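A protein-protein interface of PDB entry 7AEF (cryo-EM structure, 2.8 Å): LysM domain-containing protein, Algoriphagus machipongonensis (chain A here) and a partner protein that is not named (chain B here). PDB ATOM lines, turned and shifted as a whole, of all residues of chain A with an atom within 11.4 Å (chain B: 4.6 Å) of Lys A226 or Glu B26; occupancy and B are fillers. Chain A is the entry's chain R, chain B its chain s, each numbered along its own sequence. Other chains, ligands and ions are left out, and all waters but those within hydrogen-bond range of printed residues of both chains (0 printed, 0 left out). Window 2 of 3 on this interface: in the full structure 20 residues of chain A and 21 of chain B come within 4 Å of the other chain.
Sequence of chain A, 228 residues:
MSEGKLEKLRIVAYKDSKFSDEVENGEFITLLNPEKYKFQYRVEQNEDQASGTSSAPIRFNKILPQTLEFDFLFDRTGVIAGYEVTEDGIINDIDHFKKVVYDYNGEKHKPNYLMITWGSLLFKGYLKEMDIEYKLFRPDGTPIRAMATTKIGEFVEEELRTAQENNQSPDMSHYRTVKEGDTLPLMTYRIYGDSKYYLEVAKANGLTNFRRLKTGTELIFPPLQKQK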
ATOM      1  N   THR A 162      27.031  24.463   2.495  1.00  0.00           N
ATOM      2  CA  THR A 162      27.792  24.583   1.260  1.00  0.00           C
ATOM      3  C   THR A 162      29.240  24.995   1.492  1.00  0.00           C
ATOM      4  O   THR A 162      30.088  24.704   0.647  1.00  0.00           O
ATOM      5  CB  THR A 162      27.120  25.580   0.315  1.00  0.00           C
ATOM      6  OG1 THR A 162      26.944  26.834   0.981  1.00  0.00           O
ATOM      7  CG2 THR A 162      25.769  25.067  -0.133  1.00  0.00           C
ATOM      8  N   GLU A 165      30.764  21.523   2.643  1.00  0.00           N
ATOM      9  CA  GLU A 165      30.856  20.718   1.426  1.00  0.00           C
ATOM     10  C   GLU A 165      31.464  21.593   0.339  1.00  0.00           C
ATOM     11  O   GLU A 165      30.769  22.153  -0.513  1.00  0.00           O
ATOM     12  CB  GLU A 165      29.487  20.215   0.997  1.00  0.00           C
ATOM     13  CG  GLU A 165      28.793  19.329   1.984  1.00  0.00           C
ATOM     14  CD  GLU A 165      27.358  19.056   1.599  1.00  0.00           C
ATOM     15  OE1 GLU A 165      26.908  19.565   0.552  1.00  0.00           O
ATOM     16  OE2 GLU A 165      26.673  18.328   2.347  1.00  0.00           O
ATOM     17  N   ASN A 167      32.387  21.887  -2.650  1.00  0.00           N
ATOM     18  CA  ASN A 167      32.140  21.081  -3.837  1.00  0.00           C
ATOM     19  C   ASN A 167      32.943  21.627  -5.008  1.00  0.00           C
ATOM     20  O   ASN A 167      32.781  22.786  -5.397  1.00  0.00           O
ATOM     21  CB  ASN A 167      30.651  21.066  -4.161  1.00  0.00           C
ATOM     22  CG  ASN A 167      29.900  20.025  -3.371  1.00  0.00           C
ATOM     23  OD1 ASN A 167      30.386  18.921  -3.163  1.00  0.00           O
ATOM     24  ND2 ASN A 167      28.716  20.378  -2.913  1.00  0.00           N
ATOM     25  N   GLN A 168      33.809  20.797  -5.570  1.00  0.00           N
ATOM     26  CA  GLN A 168      34.630  21.225  -6.690  1.00  0.00           C
ATOM     27  C   GLN A 168      34.443  20.315  -7.898  1.00  0.00           C
ATOM     28  O   GLN A 168      33.572  20.553  -8.735  1.00  0.00           O
ATOM     29  CB  GLN A 168      36.096  21.269  -6.280  1.00  0.00           C
ATOM     30  CG  GLN A 168      36.794  19.936  -6.317  1.00  0.00           C
ATOM     31  CD  GLN A 168      37.977  19.894  -5.384  1.00  0.00           C
ATOM     32  OE1 GLN A 168      37.915  20.404  -4.266  1.00  0.00           O
ATOM     33  NE2 GLN A 168      39.066  19.286  -5.833  1.00  0.00           N
ATOM     34  N   PRO A 170      36.262  19.606 -13.363  1.00  0.00           N
ATOM     35  CA  PRO A 170      35.409  19.908 -14.516  1.00  0.00           C
ATOM     36  C   PRO A 170      34.473  21.100 -14.317  1.00  0.00           C
ATOM     37  O   PRO A 170      33.792  21.471 -15.264  1.00  0.00           O
ATOM     38  CB  PRO A 170      34.608  18.616 -14.691  1.00  0.00           C
ATOM     39  CG  PRO A 170      35.505  17.565 -14.205  1.00  0.00           C
ATOM     40  CD  PRO A 170      36.309  18.161 -13.085  1.00  0.00           C
ATOM     41  N   ASP A 171      34.432  21.689 -13.121  1.00  0.00           N
ATOM     42  CA  ASP A 171      33.670  22.914 -12.905  1.00  0.00           C
ATOM     43  C   ASP A 171      34.520  24.103 -12.491  1.00  0.00           C
ATOM     44  O   ASP A 171      34.120  25.242 -12.743  1.00  0.00           O
ATOM     45  CB  ASP A 171      32.578  22.705 -11.850  1.00  0.00           C
ATOM     46  CG  ASP A 171      31.352  22.021 -12.401  1.00  0.00           C
ATOM     47  OD1 ASP A 171      31.047  22.216 -13.593  1.00  0.00           O
ATOM     48  OD2 ASP A 171      30.678  21.299 -11.641  1.00  0.00           O
ATOM     49  N   MET A 172      35.673  23.886 -11.867  1.00  0.00           N
ATOM     50  CA  MET A 172      36.510  24.977 -11.384  1.00  0.00           C
ATOM     51  C   MET A 172      37.862  24.955 -12.079  1.00  0.00           C
ATOM     52  O   MET A 172      38.146  24.081 -12.900  1.00  0.00           O
ATOM     53  CB  MET A 172      36.709  24.904  -9.866  1.00  0.00           C
ATOM     54  CG  MET A 172      35.519  24.385  -9.071  1.00  0.00           C
ATOM     55  SD  MET A 172      34.043  25.414  -9.167  1.00  0.00           S
ATOM     56  CE  MET A 172      34.674  26.957  -8.543  1.00  0.00           C
ATOM     57  N   SER A 173      38.699  25.926 -11.734  1.00  0.00           N
ATOM     58  CA  SER A 173      40.038  26.030 -12.299  1.00  0.00           C
ATOM     59  C   SER A 173      41.078  25.416 -11.367  1.00  0.00           C
ATOM     60  O   SER A 173      40.891  25.336 -10.154  1.00  0.00           O
ATOM     61  CB  SER A 173      40.386  27.487 -12.565  1.00  0.00           C
ATOM     62  OG  SER A 173      39.665  27.981 -13.669  1.00  0.00           O
ATOM     63  N   TYR A 192      40.373  15.290 -15.016  1.00  0.00           N
ATOM     64  CA  TYR A 192      39.081  15.283 -15.682  1.00  0.00           C
ATOM     65  C   TYR A 192      38.387  13.931 -15.661  1.00  0.00           C
ATOM     66  O   TYR A 192      37.167  13.884 -15.830  1.00  0.00           O
ATOM     67  CB  TYR A 192      39.229  15.732 -17.142  1.00  0.00           C
ATOM     68  CG  TYR A 192      39.707  17.148 -17.305  1.00  0.00           C
ATOM     69  CD1 TYR A 192      38.842  18.215 -17.119  1.00  0.00           C
ATOM     70  CD2 TYR A 192      41.021  17.423 -17.645  1.00  0.00           C
ATOM     71  CE1 TYR A 192      39.269  19.510 -17.262  1.00  0.00           C
ATOM     72  CE2 TYR A 192      41.456  18.717 -17.792  1.00  0.00           C
ATOM     73  CZ  TYR A 192      40.575  19.757 -17.599  1.00  0.00           C
ATOM     74  OH  TYR A 192      41.000  21.051 -17.746  1.00  0.00           O
ATOM     75  N   TYR A 197      41.370  14.992 -23.343  1.00  0.00           N
ATOM     76  CA  TYR A 197      41.385  16.451 -23.363  1.00  0.00           C
ATOM     77  C   TYR A 197      42.782  17.045 -23.428  1.00  0.00           C
ATOM     78  O   TYR A 197      42.917  18.250 -23.209  1.00  0.00           O
ATOM     79  CB  TYR A 197      40.676  17.010 -22.127  1.00  0.00           C
ATOM     80  CG  TYR A 197      39.211  16.691 -22.046  1.00  0.00           C
ATOM     81  CD1 TYR A 197      38.308  17.280 -22.913  1.00  0.00           C
ATOM     82  CD2 TYR A 197      38.728  15.814 -21.090  1.00  0.00           C
ATOM     83  CE1 TYR A 197      36.969  16.997 -22.837  1.00  0.00           C
ATOM     84  CE2 TYR A 197      37.395  15.522 -21.010  1.00  0.00           C
ATOM     85  CZ  TYR A 197      36.518  16.119 -21.884  1.00  0.00           C
ATOM     86  OH  TYR A 197      35.179  15.838 -21.806  1.00  0.00           O
ATOM     87  N   PRO A 222      41.731  24.597 -17.347  1.00  0.00           N
ATOM     88  CA  PRO A 222      40.427  25.273 -17.351  1.00  0.00           C
ATOM     89  C   PRO A 222      39.279  24.294 -17.188  1.00  0.00           C
ATOM     90  O   PRO A 222      39.407  23.108 -17.523  1.00  0.00           O
ATOM     91  CB  PRO A 222      40.393  25.940 -18.736  1.00  0.00           C
ATOM     92  CG  PRO A 222      41.796  26.111 -19.088  1.00  0.00           C
ATOM     93  CD  PRO A 222      42.487  24.899 -18.567  1.00  0.00           C
ATOM     94  N   PRO A 223      38.136  24.749 -16.679  1.00  0.00           N
ATOM     95  CA  PRO A 223      36.958  23.881 -16.612  1.00  0.00           C
ATOM     96  C   PRO A 223      36.312  23.692 -17.977  1.00  0.00           C
ATOM     97  O   PRO A 223      36.556  24.433 -18.926  1.00  0.00           O
ATOM     98  CB  PRO A 223      36.026  24.636 -15.664  1.00  0.00           C
ATOM     99  CG  PRO A 223      36.400  26.046 -15.847  1.00  0.00           C
ATOM    100  CD  PRO A 223      37.879  26.053 -16.046  1.00  0.00           C
ATOM    101  N   LEU A 224      35.464  22.675 -18.057  1.00  0.00           N
ATOM    102  CA  LEU A 224      34.701  22.394 -19.265  1.00  0.00           C
ATOM    103  C   LEU A 224      33.517  23.342 -19.381  1.00  0.00           C
ATOM    104  O   LEU A 224      32.939  23.770 -18.379  1.00  0.00           O
ATOM    105  CB  LEU A 224      34.208  20.947 -19.250  1.00  0.00           C
ATOM    106  CG  LEU A 224      35.298  19.889 -19.086  1.00  0.00           C
ATOM    107  CD1 LEU A 224      34.698  18.516 -18.944  1.00  0.00           C
ATOM    108  CD2 LEU A 224      36.253  19.934 -20.253  1.00  0.00           C
ATOM    109  N   GLN A 225      33.149  23.665 -20.620  1.00  0.00           N
ATOM    110  CA  GLN A 225      32.043  24.586 -20.830  1.00  0.00           C
ATOM    111  C   GLN A 225      30.718  23.847 -20.588  1.00  0.00           C
ATOM    112  O   GLN A 225      30.624  22.625 -20.735  1.00  0.00           O
ATOM    113  CB  GLN A 225      32.048  25.161 -22.244  1.00  0.00           C
ATOM    114  CG  GLN A 225      31.907  24.162 -23.353  1.00  0.00           C
ATOM    115  CD  GLN A 225      31.969  24.805 -24.716  1.00  0.00           C
ATOM    116  OE1 GLN A 225      32.168  26.012 -24.834  1.00  0.00           O
ATOM    117  NE2 GLN A 225      31.793  24.005 -25.755  1.00  0.00           N
ATOM    118  N   LYS A 226      29.689  24.599 -20.193  1.00  0.00           N
ATOM    119  CA  LYS A 226      28.486  23.999 -19.627  1.00  0.00           C
ATOM    120  C   LYS A 226      27.326  23.902 -20.607  1.00  0.00           C
ATOM    121  O   LYS A 226      26.613  22.894 -20.608  1.00  0.00           O
ATOM    122  CB  LYS A 226      28.050  24.784 -18.391  1.00  0.00           C
ATOM    123  CG  LYS A 226      28.925  24.523 -17.184  1.00  0.00           C
ATOM    124  CD  LYS A 226      28.293  25.039 -15.908  1.00  0.00           C
ATOM    125  CE  LYS A 226      28.257  26.553 -15.878  1.00  0.00           C
ATOM    126  NZ  LYS A 226      28.427  27.063 -14.490  1.00  0.00           N
ATOM    127  N   GLN A 227      27.102  24.918 -21.430  1.00  0.00           N
ATOM    128  CA  GLN A 227      26.034  24.853 -22.420  1.00  0.00           C
ATOM    129  C   GLN A 227      26.571  24.558 -23.815  1.00  0.00           C
ATOM    130  O   GLN A 227      26.101  23.640 -24.487  1.00  0.00           O
ATOM    131  CB  GLN A 227      25.234  26.155 -22.431  1.00  0.00           C
ATOM    132  CG  GLN A 227      24.338  26.338 -21.220  1.00  0.00           C
ATOM    133  CD  GLN A 227      23.601  27.661 -21.234  1.00  0.00           C
ATOM    134  OE1 GLN A 227      23.842  28.509 -22.091  1.00  0.00           O
ATOM    135  NE2 GLN A 227      22.686  27.837 -20.293  1.00  0.00           N
ATOM    136  N   LYS B  19      22.957  19.613 -13.306  1.00  0.00           N
ATOM    137  CA  LYS B  19      22.980  21.070 -13.239  1.00  0.00           C
ATOM    138  C   LYS B  19      21.714  21.658 -13.804  1.00  0.00           C
ATOM    139  O   LYS B  19      21.145  21.158 -14.780  1.00  0.00           O
ATOM    140  CB  LYS B  19      24.127  21.695 -14.016  1.00  0.00           C
ATOM    141  CG  LYS B  19      25.486  21.294 -13.612  1.00  0.00           C
ATOM    142  CD  LYS B  19      26.512  22.065 -14.423  1.00  0.00           C
ATOM    143  CE  LYS B  19      27.928  21.658 -14.078  1.00  0.00           C
ATOM    144  NZ  LYS B  19      28.258  20.303 -14.594  1.00  0.00           N
ATOM    145  N   ILE B  20      21.283  22.753 -13.204  1.00  0.00           N
ATOM    146  CA  ILE B  20      20.140  23.486 -13.699  1.00  0.00           C
ATOM    147  C   ILE B  20      20.558  24.897 -14.009  1.00  0.00           C
ATOM    148  O   ILE B  20      21.053  25.616 -13.139  1.00  0.00           O
ATOM    149  CB  ILE B  20      18.993  23.445 -12.679  1.00  0.00           C
ATOM    150  CG1 ILE B  20      18.600  21.970 -12.455  1.00  0.00           C
ATOM    151  CG2 ILE B  20      17.837  24.289 -13.162  1.00  0.00           C
ATOM    152  CD1 ILE B  20      17.645  21.722 -11.378  1.00  0.00           C
ATOM    153  N   LEU B  21      20.393  25.278 -15.264  1.00  0.00           N
ATOM    154  CA  LEU B  21      20.802  26.586 -15.725  1.00  0.00           C
ATOM    155  C   LEU B  21      19.609  27.412 -16.116  1.00  0.00           C
ATOM    156  O   LEU B  21      18.737  26.953 -16.859  1.00  0.00           O
ATOM    157  CB  LEU B  21      21.680  26.428 -16.961  1.00  0.00           C
ATOM    158  CG  LEU B  21      22.902  25.518 -16.833  1.00  0.00           C
ATOM    159  CD1 LEU B  21      23.526  25.369 -18.173  1.00  0.00           C
ATOM    160  CD2 LEU B  21      23.869  26.090 -15.867  1.00  0.00           C
ATOM    161  N   SER B  25      22.887  30.672 -16.488  1.00  0.00           N
ATOM    162  CA  SER B  25      23.744  30.327 -15.341  1.00  0.00           C
ATOM    163  C   SER B  25      23.095  29.477 -14.257  1.00  0.00           C
ATOM    164  O   SER B  25      21.871  29.394 -14.135  1.00  0.00           O
ATOM    165  CB  SER B  25      24.280  31.593 -14.720  1.00  0.00           C
ATOM    166  OG  SER B  25      23.253  32.355 -14.163  1.00  0.00           O
ATOM    167  N   GLU B  26      23.941  28.810 -13.493  1.00  0.00           N
ATOM    168  CA  GLU B  26      23.518  27.894 -12.456  1.00  0.00           C
ATOM    169  C   GLU B  26      22.748  28.474 -11.283  1.00  0.00           C
ATOM    170  O   GLU B  26      23.135  29.476 -10.765  1.00  0.00           O
ATOM    171  CB  GLU B  26      24.755  27.160 -11.950  1.00  0.00           C
ATOM    172  CG  GLU B  26      24.523  25.695 -11.704  1.00  0.00           C
ATOM    173  CD  GLU B  26      25.752  24.949 -11.262  1.00  0.00           C
ATOM    174  OE1 GLU B  26      25.656  24.110 -10.352  1.00  0.00           O
ATOM    175  OE2 GLU B  26      26.824  25.186 -11.829  1.00  0.00           O
ATOM    176  N   ILE B  27      21.660  27.819 -10.871  1.00  0.00           N
ATOM    177  CA  ILE B  27      20.859  28.214  -9.722  1.00  0.00           C
ATOM    178  C   ILE B  27      21.764  28.015  -8.501  1.00  0.00           C
ATOM    179  O   ILE B  27      22.508  27.040  -8.467  1.00  0.00           O
ATOM    180  CB  ILE B  27      19.538  27.416  -9.647  1.00  0.00           C
ATOM    181  CG1 ILE B  27      19.801  25.902  -9.475  1.00  0.00           C
ATOM    182  CG2 ILE B  27      18.739  27.715 -10.899  1.00  0.00           C
ATOM    183  CD1 ILE B  27      18.568  25.067  -9.166  1.00  0.00           C
ATOM    184  N   PRO B  28      21.736  28.879  -7.484  1.00  0.00           N
ATOM    185  CA  PRO B  28      22.598  28.802  -6.326  1.00  0.00           C
ATOM    186  C   PRO B  28      22.448  27.514  -5.549  1.00  0.00           C
ATOM    187  O   PRO B  28      21.332  27.049  -5.302  1.00  0.00           O
ATOM    188  CB  PRO B  28      22.128  29.988  -5.489  1.00  0.00           C
ATOM    189  CG  PRO B  28      20.744  30.280  -5.975  1.00  0.00           C
ATOM    190  CD  PRO B  28      20.756  29.941  -7.435  1.00  0.00           C
ATOM    191  N   GLU B  77      17.638  25.153 -18.929  1.00  0.00           N
ATOM    192  CA  GLU B  77      18.427  24.056 -19.494  1.00  0.00           C
ATOM    193  C   GLU B  77      18.856  23.042 -18.433  1.00  0.00           C
ATOM    194  O   GLU B  77      19.355  23.384 -17.358  1.00  0.00           O
ATOM    195  CB  GLU B  77      19.642  24.575 -20.247  1.00  0.00           C
ATOM    196  CG  GLU B  77      20.495  23.493 -20.858  1.00  0.00           C
ATOM    197  CD  GLU B  77      21.609  24.026 -21.660  1.00  0.00           C
ATOM    198  OE1 GLU B  77      21.720  25.218 -21.767  1.00  0.00           O
ATOM    199  OE2 GLU B  77      22.359  23.249 -22.192  1.00  0.00           O
ATOM    200  N   THR B  79      21.085  19.523 -17.517  1.00  0.00           N
ATOM    201  CA  THR B  79      22.177  18.605 -17.875  1.00  0.00           C
ATOM    202  C   THR B  79      22.312  17.527 -16.802  1.00  0.00           C
ATOM    203  O   THR B  79      22.036  17.769 -15.625  1.00  0.00           O
ATOM    204  CB  THR B  79      23.528  19.326 -18.036  1.00  0.00           C
ATOM    205  OG1 THR B  79      23.931  19.860 -16.799  1.00  0.00           O
ATOM    206  CG2 THR B  79      23.392  20.469 -19.007  1.00  0.00           C
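OE1 of Glu B77 lies close to NE2 of Gln A227 (3.2 Å). NZ of Lys A226 lies within salt-bridge range of OE2 of Glu B26 (3.6 Å). The side-chain carboxylate (OD1) of Asp A171 lies within salt-bridge range of the side-chain amino group (NZ) of Lys B19, 3.5 Å away.
The backbone carbonyl oxygen (O) of Thr B79 lies within hydrogen-bond range of the backbone NH (N) of Lys B19 (3.1 Å). The backbone carbonyl oxygen (O) of Leu B21 is in hydrogen-bond range of the backbone NH (N) of Glu B77.
Among the printed residues, pairs that only touch across the chains: Lys A226 with Lys B19 (3.8 Å) and Gln A227 with Leu B21 (3.3 Å).
Glu B26 touches just one residue of chain A: Lys A226. Lys B19 touches just these residues of chain A: Asp A171 (3.2 Å) and Lys A226 (3.8 Å). Of the printed residues of chain A, Leu B21 touches Gln A227 (3.3 Å). No residue of chain A comes within 4 Å of Ser B25. No residue of chain A comes within 4 Å of Ile B27. Pro B28 touches none of the printed residues of chain A. Of the printed residues of chain B, Gln A227 touches Leu B21 and Glu B77. Of the printed residues of chain B, Asp A171 touches Lys B19 (3.2 Å). Printed residues of chain A within 4 Å of Glu B77: Gln A227. Glu A165 touches none of the printed residues of chain B. Asn A167 touches none of the printed residues of chain B. The nearest residue of chain A that does not touch Glu B26 is Asp A171 (5.5 Å). The nearest printed residue of chain B that does not touch Asp A171 is Glu B26 (5.5 Å).
Hydrophobic or aromatic side chains of chain B that line the printed part of chain A: Leu B21. Among the printed residues, 5 pairs touch across the chains. Among the printed residues, Asp or Glu carboxylates within 4 Å of a Lys or Arg side-chain nitrogen of the other chain: Asp A171 with Lys B19 (3.5 Å) and Lys A226 with Glu B26 (3.6 Å).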
